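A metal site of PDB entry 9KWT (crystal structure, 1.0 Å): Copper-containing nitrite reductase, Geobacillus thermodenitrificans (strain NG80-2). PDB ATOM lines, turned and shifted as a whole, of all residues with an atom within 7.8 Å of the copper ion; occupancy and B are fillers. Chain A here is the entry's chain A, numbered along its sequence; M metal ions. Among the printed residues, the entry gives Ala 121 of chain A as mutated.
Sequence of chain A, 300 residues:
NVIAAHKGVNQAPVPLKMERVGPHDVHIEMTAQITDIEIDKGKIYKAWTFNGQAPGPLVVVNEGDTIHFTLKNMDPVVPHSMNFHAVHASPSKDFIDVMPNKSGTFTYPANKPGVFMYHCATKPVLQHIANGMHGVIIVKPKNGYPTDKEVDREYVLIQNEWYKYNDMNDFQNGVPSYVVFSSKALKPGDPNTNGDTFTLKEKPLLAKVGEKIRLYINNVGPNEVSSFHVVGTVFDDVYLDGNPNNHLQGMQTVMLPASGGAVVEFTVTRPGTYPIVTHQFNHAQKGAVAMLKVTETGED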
ATOM      1  N   ALA A  32       5.826  15.795  10.252  1.00  0.00           N
ATOM      2  CA  ALA A  32       6.330  16.745   9.260  1.00  0.00           C
ATOM      3  C   ALA A  32       5.868  16.222   7.905  1.00  0.00           C
ATOM      4  O   ALA A  32       6.088  15.046   7.594  1.00  0.00           O
ATOM      5  CB  ALA A  32       7.848  16.864   9.293  1.00  0.00           C
ATOM      6  N   TRP A  48       5.833  23.142   3.514  1.00  0.00           N
ATOM      7  CA  TRP A  48       6.450  22.264   4.488  1.00  0.00           C
ATOM      8  C   TRP A  48       5.722  22.520   5.799  1.00  0.00           C
ATOM      9  O   TRP A  48       5.655  23.678   6.250  1.00  0.00           O
ATOM     10  CB  TRP A  48       7.933  22.586   4.629  1.00  0.00           C
ATOM     11  CG  TRP A  48       8.772  22.457   3.391  1.00  0.00           C
ATOM     12  CD1 TRP A  48       8.385  22.239   2.095  1.00  0.00           C
ATOM     13  CD2 TRP A  48      10.200  22.560   3.373  1.00  0.00           C
ATOM     14  NE1 TRP A  48       9.492  22.197   1.277  1.00  0.00           N
ATOM     15  CE2 TRP A  48      10.621  22.391   2.038  1.00  0.00           C
ATOM     16  CE3 TRP A  48      11.163  22.816   4.350  1.00  0.00           C
ATOM     17  CZ2 TRP A  48      11.957  22.456   1.671  1.00  0.00           C
ATOM     18  CZ3 TRP A  48      12.480  22.890   3.978  1.00  0.00           C
ATOM     19  CH2 TRP A  48      12.880  22.701   2.649  1.00  0.00           C
ATOM     20  N   THR A  49       5.169  21.473   6.402  1.00  0.00           N
ATOM     21  CA  THR A  49       4.209  21.661   7.487  1.00  0.00           C
ATOM     22  C   THR A  49       4.424  20.674   8.617  1.00  0.00           C
ATOM     23  O   THR A  49       5.000  19.596   8.436  1.00  0.00           O
ATOM     24  CB  THR A  49       2.751  21.497   7.027  1.00  0.00           C
ATOM     25  OG1 THR A  49       2.450  20.106   6.837  1.00  0.00           O
ATOM     26  CG2 THR A  49       2.463  22.276   5.764  1.00  0.00           C
ATOM     27  N   PHE A  50       3.864  21.040   9.758  1.00  0.00           N
ATOM     28  CA  PHE A  50       3.477  20.085  10.777  1.00  0.00           C
ATOM     29  C   PHE A  50       2.016  19.721  10.550  1.00  0.00           C
ATOM     30  O   PHE A  50       1.134  20.599  10.541  1.00  0.00           O
ATOM     31  CB  PHE A  50       3.670  20.680  12.170  1.00  0.00           C
ATOM     32  CG  PHE A  50       5.113  20.998  12.487  1.00  0.00           C
ATOM     33  CD1 PHE A  50       6.013  19.991  12.750  1.00  0.00           C
ATOM     34  CD2 PHE A  50       5.554  22.316  12.486  1.00  0.00           C
ATOM     35  CE1 PHE A  50       7.340  20.293  13.041  1.00  0.00           C
ATOM     36  CE2 PHE A  50       6.881  22.609  12.777  1.00  0.00           C
ATOM     37  CZ  PHE A  50       7.765  21.592  13.068  1.00  0.00           C
ATOM     38  N   LEU A  71       8.029  13.409  16.731  1.00  0.00           N
ATOM     39  CA  LEU A  71       7.875  13.877  15.355  1.00  0.00           C
ATOM     40  C   LEU A  71       8.046  12.704  14.415  1.00  0.00           C
ATOM     41  O   LEU A  71       9.078  12.033  14.442  1.00  0.00           O
ATOM     42  CB  LEU A  71       8.917  14.945  15.030  1.00  0.00           C
ATOM     43  CG  LEU A  71       8.788  15.585  13.644  1.00  0.00           C
ATOM     44  CD1 LEU A  71       7.488  16.362  13.510  1.00  0.00           C
ATOM     45  CD2 LEU A  71       9.979  16.490  13.379  1.00  0.00           C
ATOM     46  N   ASN A  73       8.469  12.024  10.611  1.00  0.00           N
ATOM     47  CA  ASN A  73       8.827  12.749   9.407  1.00  0.00           C
ATOM     48  C   ASN A  73       8.330  11.999   8.164  1.00  0.00           C
ATOM     49  O   ASN A  73       8.882  10.953   7.813  1.00  0.00           O
ATOM     50  CB  ASN A  73      10.326  13.012   9.318  1.00  0.00           C
ATOM     51  CG  ASN A  73      10.673  13.930   8.168  1.00  0.00           C
ATOM     52  OD1 ASN A  73       9.793  14.388   7.444  1.00  0.00           O
ATOM     53  ND2 ASN A  73      11.960  14.171   7.978  1.00  0.00           N
ATOM     54  N   ASP A  75       8.182  13.583   5.161  1.00  0.00           N
ATOM     55  CA  ASP A  75       8.829  14.150   3.989  1.00  0.00           C
ATOM     56  C   ASP A  75       9.732  13.088   3.371  1.00  0.00           C
ATOM     57  O   ASP A  75      10.517  12.466   4.099  1.00  0.00           O
ATOM     58  CB  ASP A  75       9.653  15.362   4.441  1.00  0.00           C
ATOM     59  CG  ASP A  75      10.250  16.189   3.301  1.00  0.00           C
ATOM     60  OD1 ASP A  75      10.745  15.596   2.305  1.00  0.00           O
ATOM     61  OD2 ASP A  75      10.266  17.436   3.419  1.00  0.00           O
ATOM     62  N   VAL A  78      13.645  15.510   2.935  1.00  0.00           N
ATOM     63  CA  VAL A  78      14.198  16.558   3.791  1.00  0.00           C
ATOM     64  C   VAL A  78      14.050  16.171   5.259  1.00  0.00           C
ATOM     65  O   VAL A  78      12.938  15.837   5.688  1.00  0.00           O
ATOM     66  CB  VAL A  78      13.568  17.935   3.528  1.00  0.00           C
ATOM     67  CG1 VAL A  78      14.341  19.016   4.270  1.00  0.00           C
ATOM     68  CG2 VAL A  78      13.507  18.253   2.044  1.00  0.00           C
ATOM     69  N   PRO A  79      15.124  16.225   6.064  1.00  0.00           N
ATOM     70  CA  PRO A  79      14.979  16.088   7.514  1.00  0.00           C
ATOM     71  C   PRO A  79      14.190  17.264   8.103  1.00  0.00           C
ATOM     72  O   PRO A  79      14.194  18.364   7.555  1.00  0.00           O
ATOM     73  CB  PRO A  79      16.421  16.103   8.025  1.00  0.00           C
ATOM     74  CG  PRO A  79      17.261  15.755   6.825  1.00  0.00           C
ATOM     75  CD  PRO A  79      16.539  16.403   5.690  1.00  0.00           C
ATOM     76  N   HIS A  80      13.546  17.016   9.245  1.00  0.00           N
ATOM     77  CA  HIS A  80      12.833  18.051   9.980  1.00  0.00           C
ATOM     78  C   HIS A  80      13.030  17.849  11.471  1.00  0.00           C
ATOM     79  O   HIS A  80      13.508  16.814  11.924  1.00  0.00           O
ATOM     80  CB  HIS A  80      11.343  18.080   9.620  1.00  0.00           C
ATOM     81  CG  HIS A  80      11.108  18.393   8.178  1.00  0.00           C
ATOM     82  ND1 HIS A  80      11.327  19.652   7.644  1.00  0.00           N
ATOM     83  CD2 HIS A  80      10.728  17.596   7.149  1.00  0.00           C
ATOM     84  CE1 HIS A  80      11.065  19.609   6.351  1.00  0.00           C
ATOM     85  NE2 HIS A  80      10.717  18.371   6.022  1.00  0.00           N
ATOM     86  N   SER A  81      12.627  18.857  12.249  1.00  0.00           N
ATOM     87  CA  SER A  81      12.869  18.864  13.682  1.00  0.00           C
ATOM     88  C   SER A  81      11.832  19.783  14.334  1.00  0.00           C
ATOM     89  O   SER A  81      10.985  20.375  13.655  1.00  0.00           O
ATOM     90  CB  SER A  81      14.273  19.381  13.994  1.00  0.00           C
ATOM     91  OG  SER A  81      14.466  20.677  13.432  1.00  0.00           O
ATOM     92  N   MET A  82      11.919  19.911  15.656  1.00  0.00           N
ATOM     93  CA  MET A  82      10.986  20.738  16.408  1.00  0.00           C
ATOM     94  C   MET A  82      11.700  21.491  17.516  1.00  0.00           C
ATOM     95  O   MET A  82      12.425  20.900  18.321  1.00  0.00           O
ATOM     96  CB  MET A  82       9.883  19.881  17.040  1.00  0.00           C
ATOM     97  CG  MET A  82       8.950  20.635  17.979  1.00  0.00           C
ATOM     98  SD  MET A  82       8.009  21.959  17.162  1.00  0.00           S
ATOM     99  CE  MET A  82       6.646  20.979  16.504  1.00  0.00           C
ATOM    100  N   ASP A  97      17.446  16.666  14.248  1.00  0.00           N
ATOM    101  CA  ASP A  97      16.733  16.230  13.067  1.00  0.00           C
ATOM    102  C   ASP A  97      16.193  14.813  13.202  1.00  0.00           C
ATOM    103  O   ASP A  97      16.790  13.930  13.822  1.00  0.00           O
ATOM    104  CB  ASP A  97      17.660  16.286  11.854  1.00  0.00           C
ATOM    105  CG  ASP A  97      17.945  17.700  11.403  1.00  0.00           C
ATOM    106  OD1 ASP A  97      17.245  18.643  11.836  1.00  0.00           O
ATOM    107  OD2 ASP A  97      18.909  17.885  10.626  1.00  0.00           O
ATOM    108  N   HIS A 119       8.522  25.826  15.986  1.00  0.00           N
ATOM    109  CA  HIS A 119       8.910  25.793  14.588  1.00  0.00           C
ATOM    110  C   HIS A 119       9.951  24.701  14.353  1.00  0.00           C
ATOM    111  O   HIS A 119      10.610  24.243  15.282  1.00  0.00           O
ATOM    112  CB  HIS A 119       9.483  27.159  14.145  1.00  0.00           C
ATOM    113  CG  HIS A 119      10.665  27.606  14.941  1.00  0.00           C
ATOM    114  ND1 HIS A 119      11.953  27.232  14.648  1.00  0.00           N
ATOM    115  CD2 HIS A 119      10.756  28.435  16.015  1.00  0.00           C
ATOM    116  CE1 HIS A 119      12.785  27.819  15.502  1.00  0.00           C
ATOM    117  NE2 HIS A 119      12.081  28.539  16.352  1.00  0.00           N
ATOM    118  N   CYS A 120      10.128  24.346  13.091  1.00  0.00           N
ATOM    119  CA  CYS A 120      11.209  23.451  12.735  1.00  0.00           C
ATOM    120  C   CYS A 120      12.551  24.151  12.965  1.00  0.00           C
ATOM    121  O   CYS A 120      12.685  25.360  12.763  1.00  0.00           O
ATOM    122  CB  CYS A 120      11.033  23.014  11.280  1.00  0.00           C
ATOM    123  SG  CYS A 120      12.333  21.927  10.684  1.00  0.00           S
ATOM    124  N   ALA A 121      13.539  23.354  13.386  1.00  0.00           N
ATOM    125  CA  ALA A 121      14.851  23.821  13.791  1.00  0.00           C
ATOM    126  C   ALA A 121      15.955  23.343  12.853  1.00  0.00           C
ATOM    127  O   ALA A 121      17.130  23.432  13.217  1.00  0.00           O
ATOM    128  CB  ALA A 121      15.154  23.370  15.233  1.00  0.00           C
ATOM    129  N   THR A 122      15.615  22.812  11.680  1.00  0.00           N
ATOM    130  CA  THR A 122      16.600  22.232  10.789  1.00  0.00           C
ATOM    131  C   THR A 122      17.243  23.312   9.929  1.00  0.00           C
ATOM    132  O   THR A 122      16.580  24.208   9.416  1.00  0.00           O
ATOM    133  CB  THR A 122      15.886  21.198   9.915  1.00  0.00           C
ATOM    134  OG1 THR A 122      15.304  20.189  10.767  1.00  0.00           O
ATOM    135  CG2 THR A 122      16.811  20.550   8.899  1.00  0.00           C
ATOM    136  N   LYS A 123      18.569  23.226   9.769  1.00  0.00           N
ATOM    137  CA  LYS A 123      19.298  24.213   8.994  1.00  0.00           C
ATOM    138  C   LYS A 123      18.996  24.030   7.501  1.00  0.00           C
ATOM    139  O   LYS A 123      18.981  22.898   6.999  1.00  0.00           O
ATOM    140  CB  LYS A 123      20.803  24.059   9.227  1.00  0.00           C
ATOM    141  CG  LYS A 123      21.693  24.948   8.359  1.00  0.00           C
ATOM    142  CD  LYS A 123      23.058  25.227   9.019  1.00  0.00           C
ATOM    143  CE  LYS A 123      24.000  25.975   8.085  1.00  0.00           C
ATOM    144  NZ  LYS A 123      25.081  25.122   7.543  1.00  0.00           N
ATOM    145  N   PRO A 124      18.781  25.123   6.747  1.00  0.00           N
ATOM    146  CA  PRO A 124      18.671  26.520   7.201  1.00  0.00           C
ATOM    147  C   PRO A 124      17.311  26.775   7.830  1.00  0.00           C
ATOM    148  O   PRO A 124      16.266  26.520   7.203  1.00  0.00           O
ATOM    149  CB  PRO A 124      18.819  27.344   5.914  1.00  0.00           C
ATOM    150  CG  PRO A 124      19.103  26.390   4.840  1.00  0.00           C
ATOM    151  CD  PRO A 124      18.704  25.031   5.283  1.00  0.00           C
ATOM    152  N   VAL A 125      17.308  27.266   9.067  1.00  0.00           N
ATOM    153  CA  VAL A 125      16.056  27.438   9.776  1.00  0.00           C
ATOM    154  C   VAL A 125      15.127  28.394   9.024  1.00  0.00           C
ATOM    155  O   VAL A 125      13.906  28.176   8.972  1.00  0.00           O
ATOM    156  CB  VAL A 125      16.314  27.878  11.230  1.00  0.00           C
ATOM    157  CG1 VAL A 125      15.021  28.189  11.955  1.00  0.00           C
ATOM    158  CG2 VAL A 125      17.088  26.785  11.970  1.00  0.00           C
ATOM    159  N   GLN A 127      14.687  28.661   5.912  1.00  0.00           N
ATOM    160  CA  GLN A 127      14.003  27.921   4.851  1.00  0.00           C
ATOM    161  C   GLN A 127      12.833  27.108   5.405  1.00  0.00           C
ATOM    162  O   GLN A 127      11.746  27.084   4.823  1.00  0.00           O
ATOM    163  CB  GLN A 127      15.012  27.008   4.141  1.00  0.00           C
ATOM    164  CG  GLN A 127      14.441  26.297   2.940  1.00  0.00           C
ATOM    165  CD  GLN A 127      15.477  25.504   2.181  1.00  0.00           C
ATOM    166  OE1 GLN A 127      16.552  25.215   2.698  1.00  0.00           O
ATOM    167  NE2 GLN A 127      15.154  25.161   0.945  1.00  0.00           N
ATOM    168  N   HIS A 128      13.059  26.411   6.518  1.00  0.00           N
ATOM    169  CA  HIS A 128      12.022  25.574   7.083  1.00  0.00           C
ATOM    170  C   HIS A 128      10.869  26.404   7.629  1.00  0.00           C
ATOM    171  O   HIS A 128       9.699  26.052   7.428  1.00  0.00           O
ATOM    172  CB  HIS A 128      12.615  24.637   8.125  1.00  0.00           C
ATOM    173  CG  HIS A 128      13.460  23.563   7.535  1.00  0.00           C
ATOM    174  ND1 HIS A 128      13.029  22.251   7.446  1.00  0.00           N
ATOM    175  CD2 HIS A 128      14.675  23.605   6.945  1.00  0.00           C
ATOM    176  CE1 HIS A 128      13.969  21.532   6.866  1.00  0.00           C
ATOM    177  NE2 HIS A 128      14.972  22.338   6.541  1.00  0.00           N
ATOM    178  N   ILE A 129      11.170  27.515   8.322  1.00  0.00           N
ATOM    179  CA  ILE A 129      10.094  28.386   8.792  1.00  0.00           C
ATOM    180  C   ILE A 129       9.353  29.001   7.613  1.00  0.00           C
ATOM    181  O   ILE A 129       8.116  28.952   7.551  1.00  0.00           O
ATOM    182  CB  ILE A 129      10.633  29.476   9.746  1.00  0.00           C
ATOM    183  CG1 ILE A 129      11.266  28.860  10.993  1.00  0.00           C
ATOM    184  CG2 ILE A 129       9.479  30.401  10.146  1.00  0.00           C
ATOM    185  CD1 ILE A 129      11.854  29.894  11.971  1.00  0.00           C
ATOM    186  N   ASN A 131       8.909  28.121   4.619  1.00  0.00           N
ATOM    187  CA  ASN A 131       8.081  27.187   3.859  1.00  0.00           C
ATOM    188  C   ASN A 131       6.869  26.682   4.619  1.00  0.00           C
ATOM    189  O   ASN A 131       6.035  25.995   4.014  1.00  0.00           O
ATOM    190  CB  ASN A 131       8.908  25.996   3.371  1.00  0.00           C
ATOM    191  CG  ASN A 131       9.745  26.318   2.139  1.00  0.00           C
ATOM    192  OD1 ASN A 131       9.347  27.089   1.261  1.00  0.00           O
ATOM    193  ND2 ASN A 131      10.895  25.687   2.048  1.00  0.00           N
ATOM    194  N   GLY A 132       6.708  27.039   5.906  1.00  0.00           N
ATOM    195  CA  GLY A 132       5.484  26.782   6.624  1.00  0.00           C
ATOM    196  C   GLY A 132       5.610  26.131   7.980  1.00  0.00           C
ATOM    197  O   GLY A 132       4.585  25.918   8.630  1.00  0.00           O
ATOM    198  N   MET A 133       6.824  25.814   8.438  1.00  0.00           N
ATOM    199  CA  MET A 133       6.990  25.009   9.654  1.00  0.00           C
ATOM    200  C   MET A 133       7.069  25.874  10.908  1.00  0.00           C
ATOM    201  O   MET A 133       8.121  26.009  11.530  1.00  0.00           O
ATOM    202  CB  MET A 133       8.151  24.037   9.545  1.00  0.00           C
ATOM    203  CG  MET A 133       8.092  23.212   8.284  1.00  0.00           C
ATOM    204  SD  MET A 133       9.207  21.788   8.200  1.00  0.00           S
ATOM    205  CE  MET A 133       8.380  20.691   9.326  1.00  0.00           C
HETATM  206 CU    CU M   1      11.702  21.339   8.654  1.00  0.00          CU
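The backbone carbonyl oxygen (O) of Val 78 lies close to a ring nitrogen (NE2) of His 80, at 3.4 Å.
OD2 of Asp 75 lies within hydrogen-bond range of NE2 of His 80.
The backbone NH (N) of His 80 sits close to the side-chain amide nitrogen (ND2) of Asn 73 (3.5 Å).
SG of Cys 120 lies close to OG1 of Thr 122.
The side-chain sulfur of Cys 120 sits close to the backbone NH of Ser 81, 3.5 Å away.
The backbone NH (N) of Met 133 lies close to the backbone carbonyl oxygen (O) of Trp 48 (3.3 Å).
The copper ion is bound by a ring nitrogen (ND1) of His 80 (2.0 Å), a ring nitrogen (ND1) of His 128 (2.0 Å), the side-chain sulfur of Cys 120 (2.2 Å) and the side-chain sulfur of Met 133 (2.6 Å).
The copper ion has four donor atoms within binding distance.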
